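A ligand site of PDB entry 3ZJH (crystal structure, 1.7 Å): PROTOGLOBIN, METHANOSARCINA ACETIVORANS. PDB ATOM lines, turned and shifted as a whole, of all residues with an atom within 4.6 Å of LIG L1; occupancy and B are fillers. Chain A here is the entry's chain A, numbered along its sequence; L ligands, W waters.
Water W4 bridges O4 of LIG L1 and OG1 of Thr 128.
Water W2 lies within hydrogen-bond range of an oxygen (O4) of LIG L1 and the guanidinium group (NH2) of Arg 92.
Water W3 lies within hydrogen-bond range of O1 of LIG L1 (2.8 Å) and O of Arg 92 (2.9 Å).
Water W1 bridges an oxygen (O3) of LIG L1 and the backbone NH of Thr 128.
O of Leu 70 touches C26 of LIG L1 (3.2 Å).
Tyr 73 touches LIG L1.
Phe 74 touches LIG L1 (CZ to C28, 3.6 Å).
CG2 of Val 89 touches C32 of LIG L1, 3.4 Å away.
Phe 93 touches LIG L1.
Trp 96 touches LIG L1.
CG1 of Ile 116 touches C11 of LIG L1 (3.9 Å).
Lys 125 touches LIG L1 (CG to O3, 3.5 Å).
Ile 137 touches LIG L1 (CD1 to C28, 3.6 Å).
Tyr 141 touches LIG L1 (O to C24, 3.2 Å).
O of Leu 142 touches C18 of LIG L1, at 3.7 Å.
Phe 145 touches LIG L1 (CD2 to C24, 3.2 Å).
Ile 146 touches LIG L1 (N to C19, 3.6 Å).
Ile 149 touches LIG L1 (CG1 to C19, 3.4 Å).
CG2 of Thr 178 touches C19 of LIG L1, at 3.8 Å.
Val 182 touches LIG L1 (CG2 to C19, 3.6 Å).
Trp 185 touches LIG L1 (CZ3 to C14, 3.4 Å).
Hydrophobic or aromatic side chains that line LIG L1: Tyr 73, Phe 74, Tyr 85, Val 89, Phe 93, Trp 96, Tyr 112, Ile 116, His 120, Ile 137, Tyr 141, Phe 145, Ile 149, Val 182 and Trp 185.
Of the 26 residues printed, 23 come within 4 Å of LIG L1.
FE1 of LIG L1 is bound by NE2 of His 120, at 2.1 Å.
O1 of LIG L1 is in hydrogen-bond range of OH of Tyr 112.
An oxygen (O3) of LIG L1 sits at hydrogen-bond distance from the side-chain hydroxyl (OH) of Tyr 85, at 2.6 Å.
The guanidinium group (NH1) of Arg 119 lies within salt-bridge range of an oxygen (O2) of LIG L1 (2.7 Å).
N of Asn 126 is in hydrogen-bond range of O3 of LIG L1 (2.8 Å).
NE of Arg 92 is in salt-bridge range of O2 of LIG L1.
O of His 120 sits at hydrogen-bond distance from N of Ile 137, at 3.1 Å.
A ring nitrogen (ND1) of His 120 lies within hydrogen-bond range of the backbone carbonyl oxygen (O) of Ile 116, at 2.9 Å.
The guanidinium group (NH1) of Arg 119 sits at hydrogen-bond distance from the side-chain hydroxyl (OH) of Tyr 112 (3.3 Å).
The side-chain hydroxyl (OH) of Tyr 85 lies within hydrogen-bond range of the side-chain amide oxygen (OD1) of Asn 126, 3.2 Å away.
OH of Tyr 85 sits at hydrogen-bond distance from NZ of Lys 125, 3.1 Å away.
The guanidinium group of Arg 119 is in hydrogen-bond range of the side-chain hydroxyl of Thr 128, 3.2 Å away.
OD1 of Asn 126 lies within hydrogen-bond range of NZ of Lys 125.
O of Tyr 73 is in hydrogen-bond range of NZ of Lys 125, at 3.0 Å.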
ATOM      1  N   TYR A   9      37.576 -21.738   5.052  1.00  0.00           N
ATOM      2  CA  TYR A   9      37.710 -20.383   5.610  1.00  0.00           C
ATOM      3  C   TYR A   9      38.703 -19.575   4.798  1.00  0.00           C
ATOM      4  O   TYR A   9      39.866 -19.961   4.658  1.00  0.00           O
ATOM      5  CB  TYR A   9      38.193 -20.491   7.059  1.00  0.00           C
ATOM      6  CG  TYR A   9      38.370 -19.175   7.767  1.00  0.00           C
ATOM      7  CD1 TYR A   9      37.265 -18.452   8.205  1.00  0.00           C
ATOM      8  CD2 TYR A   9      39.632 -18.651   8.007  1.00  0.00           C
ATOM      9  CE1 TYR A   9      37.409 -17.250   8.871  1.00  0.00           C
ATOM     10  CE2 TYR A   9      39.799 -17.454   8.679  1.00  0.00           C
ATOM     11  CZ  TYR A   9      38.677 -16.757   9.103  1.00  0.00           C
ATOM     12  OH  TYR A   9      38.835 -15.561   9.787  1.00  0.00           O
ATOM     13  N   VAL A  64      19.022 -24.936  16.203  1.00  0.00           N
ATOM     14  CA  VAL A  64      18.811 -25.316  14.802  1.00  0.00           C
ATOM     15  C   VAL A  64      18.288 -26.738  14.683  1.00  0.00           C
ATOM     16  O   VAL A  64      17.361 -27.020  13.911  1.00  0.00           O
ATOM     17  CB  VAL A  64      20.089 -25.155  13.964  1.00  0.00           C
ATOM     18  CG1 VAL A  64      19.829 -25.611  12.538  1.00  0.00           C
ATOM     19  CG2 VAL A  64      20.533 -23.670  13.944  1.00  0.00           C
ATOM     20  N   LEU A  70      14.667 -25.469  10.149  1.00  0.00           N
ATOM     21  CA  LEU A  70      15.975 -24.802  10.233  1.00  0.00           C
ATOM     22  C   LEU A  70      17.085 -25.811   9.939  1.00  0.00           C
ATOM     23  O   LEU A  70      17.992 -25.526   9.159  1.00  0.00           O
ATOM     24  CB  LEU A  70      16.182 -24.176  11.627  1.00  0.00           C
ATOM     25  CG  LEU A  70      15.080 -23.177  12.023  1.00  0.00           C
ATOM     26  CD1 LEU A  70      15.423 -22.561  13.408  1.00  0.00           C
ATOM     27  CD2 LEU A  70      14.999 -22.096  10.985  1.00  0.00           C
ATOM     28  N   TYR A  73      18.310 -26.652   6.316  1.00  0.00           N
ATOM     29  CA  TYR A  73      19.312 -25.998   5.480  1.00  0.00           C
ATOM     30  C   TYR A  73      20.656 -26.710   5.494  1.00  0.00           C
ATOM     31  O   TYR A  73      21.522 -26.407   4.677  1.00  0.00           O
ATOM     32  CB  TYR A  73      19.432 -24.510   5.821  1.00  0.00           C
ATOM     33  CG  TYR A  73      18.144 -23.820   5.496  1.00  0.00           C
ATOM     34  CD1 TYR A  73      17.781 -23.613   4.151  1.00  0.00           C
ATOM     35  CD2 TYR A  73      17.250 -23.434   6.502  1.00  0.00           C
ATOM     36  CE1 TYR A  73      16.579 -23.027   3.826  1.00  0.00           C
ATOM     37  CE2 TYR A  73      16.041 -22.859   6.180  1.00  0.00           C
ATOM     38  CZ  TYR A  73      15.710 -22.655   4.841  1.00  0.00           C
ATOM     39  OH  TYR A  73      14.508 -22.080   4.497  1.00  0.00           O
ATOM     40  N   PHE A  74      20.815 -27.659   6.424  1.00  0.00           N
ATOM     41  CA  PHE A  74      21.992 -28.531   6.470  1.00  0.00           C
ATOM     42  C   PHE A  74      21.710 -29.922   5.907  1.00  0.00           C
ATOM     43  O   PHE A  74      22.572 -30.794   5.988  1.00  0.00           O
ATOM     44  CB  PHE A  74      22.507 -28.653   7.906  1.00  0.00           C
ATOM     45  CG  PHE A  74      23.145 -27.399   8.424  1.00  0.00           C
ATOM     46  CD1 PHE A  74      24.495 -27.149   8.206  1.00  0.00           C
ATOM     47  CD2 PHE A  74      22.407 -26.484   9.145  1.00  0.00           C
ATOM     48  CE1 PHE A  74      25.077 -26.004   8.683  1.00  0.00           C
ATOM     49  CE2 PHE A  74      23.000 -25.335   9.631  1.00  0.00           C
ATOM     50  CZ  PHE A  74      24.319 -25.094   9.397  1.00  0.00           C
ATOM     51  N   TYR A  85      28.692 -31.611   6.429  1.00  0.00           N
ATOM     52  CA  TYR A  85      28.328 -30.206   6.248  1.00  0.00           C
ATOM     53  C   TYR A  85      28.261 -29.504   7.600  1.00  0.00           C
ATOM     54  O   TYR A  85      28.859 -28.449   7.802  1.00  0.00           O
ATOM     55  CB  TYR A  85      26.965 -30.169   5.592  1.00  0.00           C
ATOM     56  CG  TYR A  85      26.520 -28.872   4.968  1.00  0.00           C
ATOM     57  CD1 TYR A  85      27.396 -27.808   4.732  1.00  0.00           C
ATOM     58  CD2 TYR A  85      25.195 -28.712   4.577  1.00  0.00           C
ATOM     59  CE1 TYR A  85      26.949 -26.635   4.112  1.00  0.00           C
ATOM     60  CE2 TYR A  85      24.743 -27.559   3.969  1.00  0.00           C
ATOM     61  CZ  TYR A  85      25.608 -26.527   3.750  1.00  0.00           C
ATOM     62  OH  TYR A  85      25.118 -25.395   3.130  1.00  0.00           O
ATOM     63  N   VAL A  89      30.860 -26.413   8.770  1.00  0.00           N
ATOM     64  CA  VAL A  89      30.285 -25.085   9.024  1.00  0.00           C
ATOM     65  C   VAL A  89      30.502 -24.689  10.483  1.00  0.00           C
ATOM     66  O   VAL A  89      30.792 -23.535  10.777  1.00  0.00           O
ATOM     67  CB  VAL A  89      28.796 -25.043   8.680  1.00  0.00           C
ATOM     68  CG1 VAL A  89      28.119 -23.759   9.197  1.00  0.00           C
ATOM     69  CG2 VAL A  89      28.617 -25.211   7.129  1.00  0.00           C
ATOM     70  N   ARG A  92      33.819 -23.074  10.938  1.00  0.00           N
ATOM     71  CA  ARG A  92      33.802 -21.708  10.418  1.00  0.00           C
ATOM     72  C   ARG A  92      32.989 -20.740  11.255  1.00  0.00           C
ATOM     73  O   ARG A  92      33.332 -19.565  11.397  1.00  0.00           O
ATOM     74  CB  ARG A  92      33.426 -21.692   8.924  1.00  0.00           C
ATOM     75  CG  ARG A  92      34.457 -22.434   8.082  1.00  0.00           C
ATOM     76  CD  ARG A  92      34.331 -22.113   6.569  1.00  0.00           C
ATOM     77  NE  ARG A  92      33.035 -22.485   6.011  1.00  0.00           N
ATOM     78  CZ  ARG A  92      32.706 -23.712   5.578  1.00  0.00           C
ATOM     79  NH1 ARG A  92      33.565 -24.720   5.644  1.00  0.00           N
ATOM     80  NH2 ARG A  92      31.501 -23.922   5.101  1.00  0.00           N
ATOM     81  N   PHE A  93      31.897 -21.240  11.822  1.00  0.00           N
ATOM     82  CA  PHE A  93      31.086 -20.391  12.702  1.00  0.00           C
ATOM     83  C   PHE A  93      31.883 -20.089  13.968  1.00  0.00           C
ATOM     84  O   PHE A  93      31.863 -18.971  14.473  1.00  0.00           O
ATOM     85  CB  PHE A  93      29.761 -21.101  13.021  1.00  0.00           C
ATOM     86  CG  PHE A  93      28.820 -20.278  13.832  1.00  0.00           C
ATOM     87  CD1 PHE A  93      28.949 -20.196  15.217  1.00  0.00           C
ATOM     88  CD2 PHE A  93      27.787 -19.593  13.218  1.00  0.00           C
ATOM     89  CE1 PHE A  93      28.063 -19.427  15.975  1.00  0.00           C
ATOM     90  CE2 PHE A  93      26.887 -18.817  13.967  1.00  0.00           C
ATOM     91  CZ  PHE A  93      27.029 -18.743  15.351  1.00  0.00           C
ATOM     92  N   TRP A  96      34.122 -17.328  13.154  1.00  0.00           N
ATOM     93  CA  TRP A  96      33.317 -16.102  13.075  1.00  0.00           C
ATOM     94  C   TRP A  96      33.098 -15.415  14.430  1.00  0.00           C
ATOM     95  O   TRP A  96      33.134 -14.180  14.548  1.00  0.00           O
ATOM     96  CB  TRP A  96      31.958 -16.416  12.408  1.00  0.00           C
ATOM     97  CG  TRP A  96      31.029 -15.275  12.408  1.00  0.00           C
ATOM     98  CD1 TRP A  96      31.021 -14.226  11.517  1.00  0.00           C
ATOM     99  CD2 TRP A  96      29.967 -15.038  13.333  1.00  0.00           C
ATOM    100  NE1 TRP A  96      30.012 -13.365  11.845  1.00  0.00           N
ATOM    101  CE2 TRP A  96      29.352 -13.823  12.945  1.00  0.00           C
ATOM    102  CE3 TRP A  96      29.487 -15.731  14.446  1.00  0.00           C
ATOM    103  CZ2 TRP A  96      28.257 -13.284  13.637  1.00  0.00           C
ATOM    104  CZ3 TRP A  96      28.392 -15.191  15.138  1.00  0.00           C
ATOM    105  CH2 TRP A  96      27.795 -13.984  14.728  1.00  0.00           C
ATOM    106  N   TYR A 112      34.809 -10.299   3.297  1.00  0.00           N
ATOM    107  CA  TYR A 112      34.376 -11.607   3.812  1.00  0.00           C
ATOM    108  C   TYR A 112      32.902 -11.577   4.159  1.00  0.00           C
ATOM    109  O   TYR A 112      32.217 -12.593   4.046  1.00  0.00           O
ATOM    110  CB  TYR A 112      35.216 -12.105   5.011  1.00  0.00           C
ATOM    111  CG  TYR A 112      35.187 -13.618   5.118  1.00  0.00           C
ATOM    112  CD1 TYR A 112      35.664 -14.405   4.064  1.00  0.00           C
ATOM    113  CD2 TYR A 112      34.671 -14.276   6.252  1.00  0.00           C
ATOM    114  CE1 TYR A 112      35.634 -15.798   4.136  1.00  0.00           C
ATOM    115  CE2 TYR A 112      34.638 -15.671   6.305  1.00  0.00           C
ATOM    116  CZ  TYR A 112      35.128 -16.413   5.264  1.00  0.00           C
ATOM    117  OH  TYR A 112      35.105 -17.794   5.334  1.00  0.00           O
ATOM    118  N   ILE A 116      30.314 -14.351   3.042  1.00  0.00           N
ATOM    119  CA  ILE A 116      29.407 -15.123   3.919  1.00  0.00           C
ATOM    120  C   ILE A 116      27.953 -14.999   3.459  1.00  0.00           C
ATOM    121  O   ILE A 116      27.203 -15.970   3.452  1.00  0.00           O
ATOM    122  CB  ILE A 116      29.519 -14.656   5.405  1.00  0.00           C
ATOM    123  CG1 ILE A 116      30.925 -14.940   5.931  1.00  0.00           C
ATOM    124  CG2 ILE A 116      28.430 -15.368   6.270  1.00  0.00           C
ATOM    125  CD1 ILE A 116      31.187 -14.425   7.319  1.00  0.00           C
ATOM    126  N   ARG A 119      27.454 -17.278   0.589  1.00  0.00           N
ATOM    127  CA  ARG A 119      27.451 -18.690   0.985  1.00  0.00           C
ATOM    128  C   ARG A 119      26.103 -19.123   1.601  1.00  0.00           C
ATOM    129  O   ARG A 119      25.736 -20.300   1.503  1.00  0.00           O
ATOM    130  CB  ARG A 119      28.579 -18.961   1.976  1.00  0.00           C
ATOM    131  CG  ARG A 119      29.926 -18.962   1.339  1.00  0.00           C
ATOM    132  CD  ARG A 119      31.044 -19.184   2.335  1.00  0.00           C
ATOM    133  NE  ARG A 119      32.306 -19.036   1.632  1.00  0.00           N
ATOM    134  CZ  ARG A 119      33.482 -19.400   2.098  1.00  0.00           C
ATOM    135  NH1 ARG A 119      33.565 -19.930   3.326  1.00  0.00           N
ATOM    136  NH2 ARG A 119      34.565 -19.225   1.356  1.00  0.00           N
ATOM    137  N   HIS A 120      25.396 -18.217   2.247  1.00  0.00           N
ATOM    138  CA  HIS A 120      24.035 -18.533   2.688  1.00  0.00           C
ATOM    139  C   HIS A 120      23.101 -18.531   1.508  1.00  0.00           C
ATOM    140  O   HIS A 120      22.108 -19.251   1.497  1.00  0.00           O
ATOM    141  CB  HIS A 120      23.534 -17.545   3.743  1.00  0.00           C
ATOM    142  CG  HIS A 120      24.162 -17.731   5.089  1.00  0.00           C
ATOM    143  ND1 HIS A 120      25.412 -17.234   5.405  1.00  0.00           N
ATOM    144  CD2 HIS A 120      23.725 -18.393   6.192  1.00  0.00           C
ATOM    145  CE1 HIS A 120      25.707 -17.578   6.653  1.00  0.00           C
ATOM    146  NE2 HIS A 120      24.701 -18.292   7.140  1.00  0.00           N
ATOM    147  N   LYS A 125      25.970 -21.227  -1.828  1.00  0.00           N
ATOM    148  CA  LYS A 125      25.668 -22.259  -0.844  1.00  0.00           C
ATOM    149  C   LYS A 125      26.046 -23.646  -1.369  1.00  0.00           C
ATOM    150  O   LYS A 125      25.807 -23.962  -2.539  1.00  0.00           O
ATOM    151  CB  LYS A 125      24.186 -22.235  -0.425  1.00  0.00           C
ATOM    152  CG  LYS A 125      23.882 -23.246   0.699  1.00  0.00           C
ATOM    153  CD  LYS A 125      22.404 -23.167   1.152  1.00  0.00           C
ATOM    154  CE  LYS A 125      22.095 -24.136   2.303  1.00  0.00           C
ATOM    155  NZ  LYS A 125      22.292 -25.596   1.904  1.00  0.00           N
ATOM    156  N   ASN A 126      26.632 -24.467  -0.503  1.00  0.00           N
ATOM    157  CA  ASN A 126      27.016 -25.854  -0.805  1.00  0.00           C
ATOM    158  C   ASN A 126      28.297 -26.009  -1.607  1.00  0.00           C
ATOM    159  O   ASN A 126      28.725 -27.122  -1.835  1.00  0.00           O
ATOM    160  CB  ASN A 126      25.942 -26.587  -1.626  1.00  0.00           C
ATOM    161  CG  ASN A 126      24.581 -26.516  -0.975  1.00  0.00           C
ATOM    162  OD1 ASN A 126      24.474 -26.658   0.245  1.00  0.00           O
ATOM    163  ND2 ASN A 126      23.546 -26.278  -1.762  1.00  0.00           N
ATOM    164  N   THR A 128      31.356 -24.399  -0.841  1.00  0.00           N
ATOM    165  CA  THR A 128      32.552 -24.399  -0.013  1.00  0.00           C
ATOM    166  C   THR A 128      32.897 -25.826   0.458  1.00  0.00           C
ATOM    167  O   THR A 128      34.062 -26.273   0.437  1.00  0.00           O
ATOM    168  CB  THR A 128      32.405 -23.422   1.156  1.00  0.00           C
ATOM    169  OG1 THR A 128      32.186 -22.095   0.618  1.00  0.00           O
ATOM    170  CG2 THR A 128      33.632 -23.419   2.050  1.00  0.00           C
ATOM    171  N   ILE A 137      19.249 -20.528   1.446  1.00  0.00           N
ATOM    172  CA  ILE A 137      18.655 -20.295   2.743  1.00  0.00           C
ATOM    173  C   ILE A 137      17.787 -19.064   2.663  1.00  0.00           C
ATOM    174  O   ILE A 137      18.274 -17.937   2.425  1.00  0.00           O
ATOM    175  CB  ILE A 137      19.687 -20.124   3.869  1.00  0.00           C
ATOM    176  CG1 ILE A 137      20.608 -21.353   3.952  1.00  0.00           C
ATOM    177  CG2 ILE A 137      18.971 -19.835   5.197  1.00  0.00           C
ATOM    178  CD1 ILE A 137      21.890 -21.080   4.726  1.00  0.00           C
ATOM    179  N   TYR A 141      14.982 -16.044   7.255  1.00  0.00           N
ATOM    180  CA  TYR A 141      15.583 -16.726   8.397  1.00  0.00           C
ATOM    181  C   TYR A 141      16.937 -16.127   8.788  1.00  0.00           C
ATOM    182  O   TYR A 141      17.323 -16.158   9.947  1.00  0.00           O
ATOM    183  CB  TYR A 141      15.717 -18.232   8.124  1.00  0.00           C
ATOM    184  CG  TYR A 141      14.371 -18.930   8.017  1.00  0.00           C
ATOM    185  CD1 TYR A 141      13.456 -18.885   9.066  1.00  0.00           C
ATOM    186  CD2 TYR A 141      14.018 -19.613   6.854  1.00  0.00           C
ATOM    187  CE1 TYR A 141      12.235 -19.521   8.985  1.00  0.00           C
ATOM    188  CE2 TYR A 141      12.772 -20.246   6.747  1.00  0.00           C
ATOM    189  CZ  TYR A 141      11.887 -20.182   7.819  1.00  0.00           C
ATOM    190  OH  TYR A 141      10.661 -20.787   7.746  1.00  0.00           O
ATOM    191  N   LEU A 142      17.668 -15.569   7.818  1.00  0.00           N
ATOM    192  CA  LEU A 142      18.876 -14.783   8.147  1.00  0.00           C
ATOM    193  C   LEU A 142      18.551 -13.609   9.075  1.00  0.00           C
ATOM    194  O   LEU A 142      19.201 -13.423  10.110  1.00  0.00           O
ATOM    195  CB  LEU A 142      19.555 -14.251   6.883  1.00  0.00           C
ATOM    196  CG  LEU A 142      20.700 -15.144   6.397  1.00  0.00           C
ATOM    197  CD1 LEU A 142      20.081 -16.499   5.979  1.00  0.00           C
ATOM    198  CD2 LEU A 142      21.478 -14.478   5.226  1.00  0.00           C
ATOM    199  N   PHE A 145      17.434 -14.882  12.508  1.00  0.00           N
ATOM    200  CA  PHE A 145      18.499 -15.448  13.348  1.00  0.00           C
ATOM    201  C   PHE A 145      19.349 -14.425  14.087  1.00  0.00           C
ATOM    202  O   PHE A 145      20.126 -14.788  14.965  1.00  0.00           O
ATOM    203  CB  PHE A 145      19.428 -16.327  12.515  1.00  0.00           C
ATOM    204  CG  PHE A 145      19.044 -17.780  12.502  1.00  0.00           C
ATOM    205  CD1 PHE A 145      17.697 -18.159  12.512  1.00  0.00           C
ATOM    206  CD2 PHE A 145      20.025 -18.756  12.476  1.00  0.00           C
ATOM    207  CE1 PHE A 145      17.335 -19.535  12.487  1.00  0.00           C
ATOM    208  CE2 PHE A 145      19.699 -20.114  12.444  1.00  0.00           C
ATOM    209  CZ  PHE A 145      18.345 -20.517  12.437  1.00  0.00           C
ATOM    210  N   ILE A 146      19.222 -13.143  13.734  1.00  0.00           N
ATOM    211  CA  ILE A 146      19.832 -12.097  14.555  1.00  0.00           C
ATOM    212  C   ILE A 146      19.436 -12.321  15.998  1.00  0.00           C
ATOM    213  O   ILE A 146      20.269 -12.163  16.910  1.00  0.00           O
ATOM    214  CB  ILE A 146      19.393 -10.679  14.129  1.00  0.00           C
ATOM    215  CG1 ILE A 146      19.952 -10.362  12.733  1.00  0.00           C
ATOM    216  CG2 ILE A 146      19.922  -9.625  15.163  1.00  0.00           C
ATOM    217  CD1 ILE A 146      19.257  -9.201  12.047  1.00  0.00           C
ATOM    218  N   ILE A 149      21.073 -15.743  17.573  1.00  0.00           N
ATOM    219  CA  ILE A 149      22.495 -15.592  17.711  1.00  0.00           C
ATOM    220  C   ILE A 149      22.810 -14.737  18.941  1.00  0.00           C
ATOM    221  O   ILE A 149      23.626 -15.114  19.784  1.00  0.00           O
ATOM    222  CB  ILE A 149      23.133 -15.029  16.439  1.00  0.00           C
ATOM    223  CG1 ILE A 149      22.942 -16.014  15.278  1.00  0.00           C
ATOM    224  CG2 ILE A 149      24.590 -14.704  16.705  1.00  0.00           C
ATOM    225  CD1 ILE A 149      23.239 -17.474  15.607  1.00  0.00           C
ATOM    226  N   THR A 178      26.039  -8.165  15.080  1.00  0.00           N
ATOM    227  CA  THR A 178      25.329  -9.225  14.387  1.00  0.00           C
ATOM    228  C   THR A 178      24.333  -8.613  13.400  1.00  0.00           C
ATOM    229  O   THR A 178      24.204  -9.077  12.251  1.00  0.00           O
ATOM    230  CB  THR A 178      24.615 -10.156  15.397  1.00  0.00           C
ATOM    231  OG1 THR A 178      25.593 -10.754  16.232  1.00  0.00           O
ATOM    232  CG2 THR A 178      23.823 -11.248  14.668  1.00  0.00           C
ATOM    233  N   VAL A 182      24.296  -9.102   9.274  1.00  0.00           N
ATOM    234  CA  VAL A 182      23.157  -9.587   8.514  1.00  0.00           C
ATOM    235  C   VAL A 182      22.674  -8.547   7.507  1.00  0.00           C
ATOM    236  O   VAL A 182      22.288  -8.875   6.369  1.00  0.00           O
ATOM    237  CB  VAL A 182      22.042 -10.084   9.449  1.00  0.00           C
ATOM    238  CG1 VAL A 182      20.790 -10.391   8.685  1.00  0.00           C
ATOM    239  CG2 VAL A 182      22.548 -11.291  10.248  1.00  0.00           C
ATOM    240  N   TRP A 185      24.820  -8.994   4.644  1.00  0.00           N
ATOM    241  CA  TRP A 185      24.595 -10.239   3.935  1.00  0.00           C
ATOM    242  C   TRP A 185      23.343 -10.215   3.051  1.00  0.00           C
ATOM    243  O   TRP A 185      23.176 -11.088   2.189  1.00  0.00           O
ATOM    244  CB  TRP A 185      24.522 -11.436   4.885  1.00  0.00           C
ATOM    245  CG  TRP A 185      25.715 -11.596   5.793  1.00  0.00           C
ATOM    246  CD1 TRP A 185      26.892 -10.887   5.769  1.00  0.00           C
ATOM    247  CD2 TRP A 185      25.820 -12.513   6.879  1.00  0.00           C
ATOM    248  NE1 TRP A 185      27.727 -11.318   6.778  1.00  0.00           N
ATOM    249  CE2 TRP A 185      27.099 -12.318   7.469  1.00  0.00           C
ATOM    250  CE3 TRP A 185      24.987 -13.513   7.396  1.00  0.00           C
ATOM    251  CZ2 TRP A 185      27.532 -13.064   8.571  1.00  0.00           C
ATOM    252  CZ3 TRP A 185      25.413 -14.241   8.486  1.00  0.00           C
ATOM    253  CH2 TRP A 185      26.673 -14.021   9.056  1.00  0.00           C
HETATM  254  C1  LIG L   1      27.303 -20.679   7.231  1.00  0.00           C
HETATM  255  C2  LIG L   1      26.704 -17.376  10.798  1.00  0.00           C
HETATM  256  C3  LIG L   1      21.999 -17.438   9.638  1.00  0.00           C
HETATM  257  C4  LIG L   1      22.722 -22.004   8.180  1.00  0.00           C
HETATM  258  C5  LIG L   1      27.583 -19.749   8.223  1.00  0.00           C
HETATM  259  C6  LIG L   1      28.889 -19.293   8.637  1.00  0.00           C
HETATM  260  C7  LIG L   1      28.713 -18.379   9.614  1.00  0.00           C
HETATM  261  C8  LIG L   1      27.299 -18.229   9.867  1.00  0.00           C
HETATM  262  C9  LIG L   1      29.808 -17.594  10.386  1.00  0.00           C
HETATM  263  C10 LIG L   1      30.240 -19.755   8.033  1.00  0.00           C
HETATM  264  C11 LIG L   1      30.774 -18.619   7.146  1.00  0.00           C
HETATM  265  C12 LIG L   1      32.009 -19.078   6.405  1.00  0.00           C
HETATM  266  O1  LIG L   1      33.137 -18.676   6.800  1.00  0.00           O
HETATM  267  O2  LIG L   1      31.861 -19.842   5.426  1.00  0.00           O
HETATM  268  C13 LIG L   1      25.375 -17.005  10.730  1.00  0.00           C
HETATM  269  C14 LIG L   1      24.734 -15.877  11.382  1.00  0.00           C
HETATM  270  C15 LIG L   1      23.428 -15.903  11.050  1.00  0.00           C
HETATM  271  C16 LIG L   1      23.198 -17.049  10.187  1.00  0.00           C
HETATM  272  C17 LIG L   1      25.436 -14.825  12.270  1.00  0.00           C
HETATM  273  C18 LIG L   1      22.334 -14.882  11.453  1.00  0.00           C
HETATM  274  C19 LIG L   1      22.448 -14.117  12.538  1.00  0.00           C
HETATM  275  C20 LIG L   1      21.753 -18.725   9.241  1.00  0.00           C
HETATM  276  C21 LIG L   1      20.465 -19.398   9.144  1.00  0.00           C
HETATM  277  C22 LIG L   1      20.690 -20.666   8.740  1.00  0.00           C
HETATM  278  C23 LIG L   1      22.098 -20.850   8.593  1.00  0.00           C
HETATM  279  C24 LIG L   1      19.097 -18.740   9.414  1.00  0.00           C
HETATM  280  C25 LIG L   1      19.675 -21.791   8.493  1.00  0.00           C
HETATM  281  C26 LIG L   1      19.793 -22.901   9.214  1.00  0.00           C
HETATM  282  C27 LIG L   1      23.966 -22.004   7.609  1.00  0.00           C
HETATM  283  C28 LIG L   1      24.401 -22.913   6.574  1.00  0.00           C
HETATM  284  C29 LIG L   1      25.836 -22.495   6.274  1.00  0.00           C
HETATM  285  C30 LIG L   1      26.112 -21.371   7.132  1.00  0.00           C
HETATM  286  C31 LIG L   1      23.581 -24.057   5.916  1.00  0.00           C
HETATM  287  C32 LIG L   1      26.773 -23.113   5.216  1.00  0.00           C
HETATM  288  C33 LIG L   1      26.525 -22.307   3.929  1.00  0.00           C
HETATM  289  C34 LIG L   1      27.407 -22.848   2.830  1.00  0.00           C
HETATM  290  O3  LIG L   1      26.987 -23.837   2.159  1.00  0.00           O
HETATM  291  O4  LIG L   1      28.545 -22.304   2.659  1.00  0.00           O
HETATM  292  N1  LIG L   1      26.642 -19.093   9.002  1.00  0.00           N
HETATM  293  N2  LIG L   1      24.407 -17.703  10.031  1.00  0.00           N
HETATM  294  N3  LIG L   1      22.709 -19.640   8.897  1.00  0.00           N
HETATM  295  N4  LIG L   1      24.988 -21.110   7.901  1.00  0.00           N
HETATM  296 FE1  LIG L   1      24.692 -19.368   8.891  1.00  0.00          FE
HETATM  297  C1  LG2 L   2      24.721 -20.598  10.787  1.00  0.00           C
HETATM  298  N1  LG2 L   2      25.231 -21.378  11.495  1.00  0.00           N
HETATM  299  O   HOH W   1      29.366 -25.509   1.681  1.00  0.00           O
HETATM  300  O   HOH W   2      29.780 -21.620   4.947  1.00  0.00           O
HETATM  301  O   HOH W   3      33.734 -17.619   9.308  1.00  0.00           O
HETATM  302  O   HOH W   4      29.469 -22.380   0.190  1.00  0.00           O
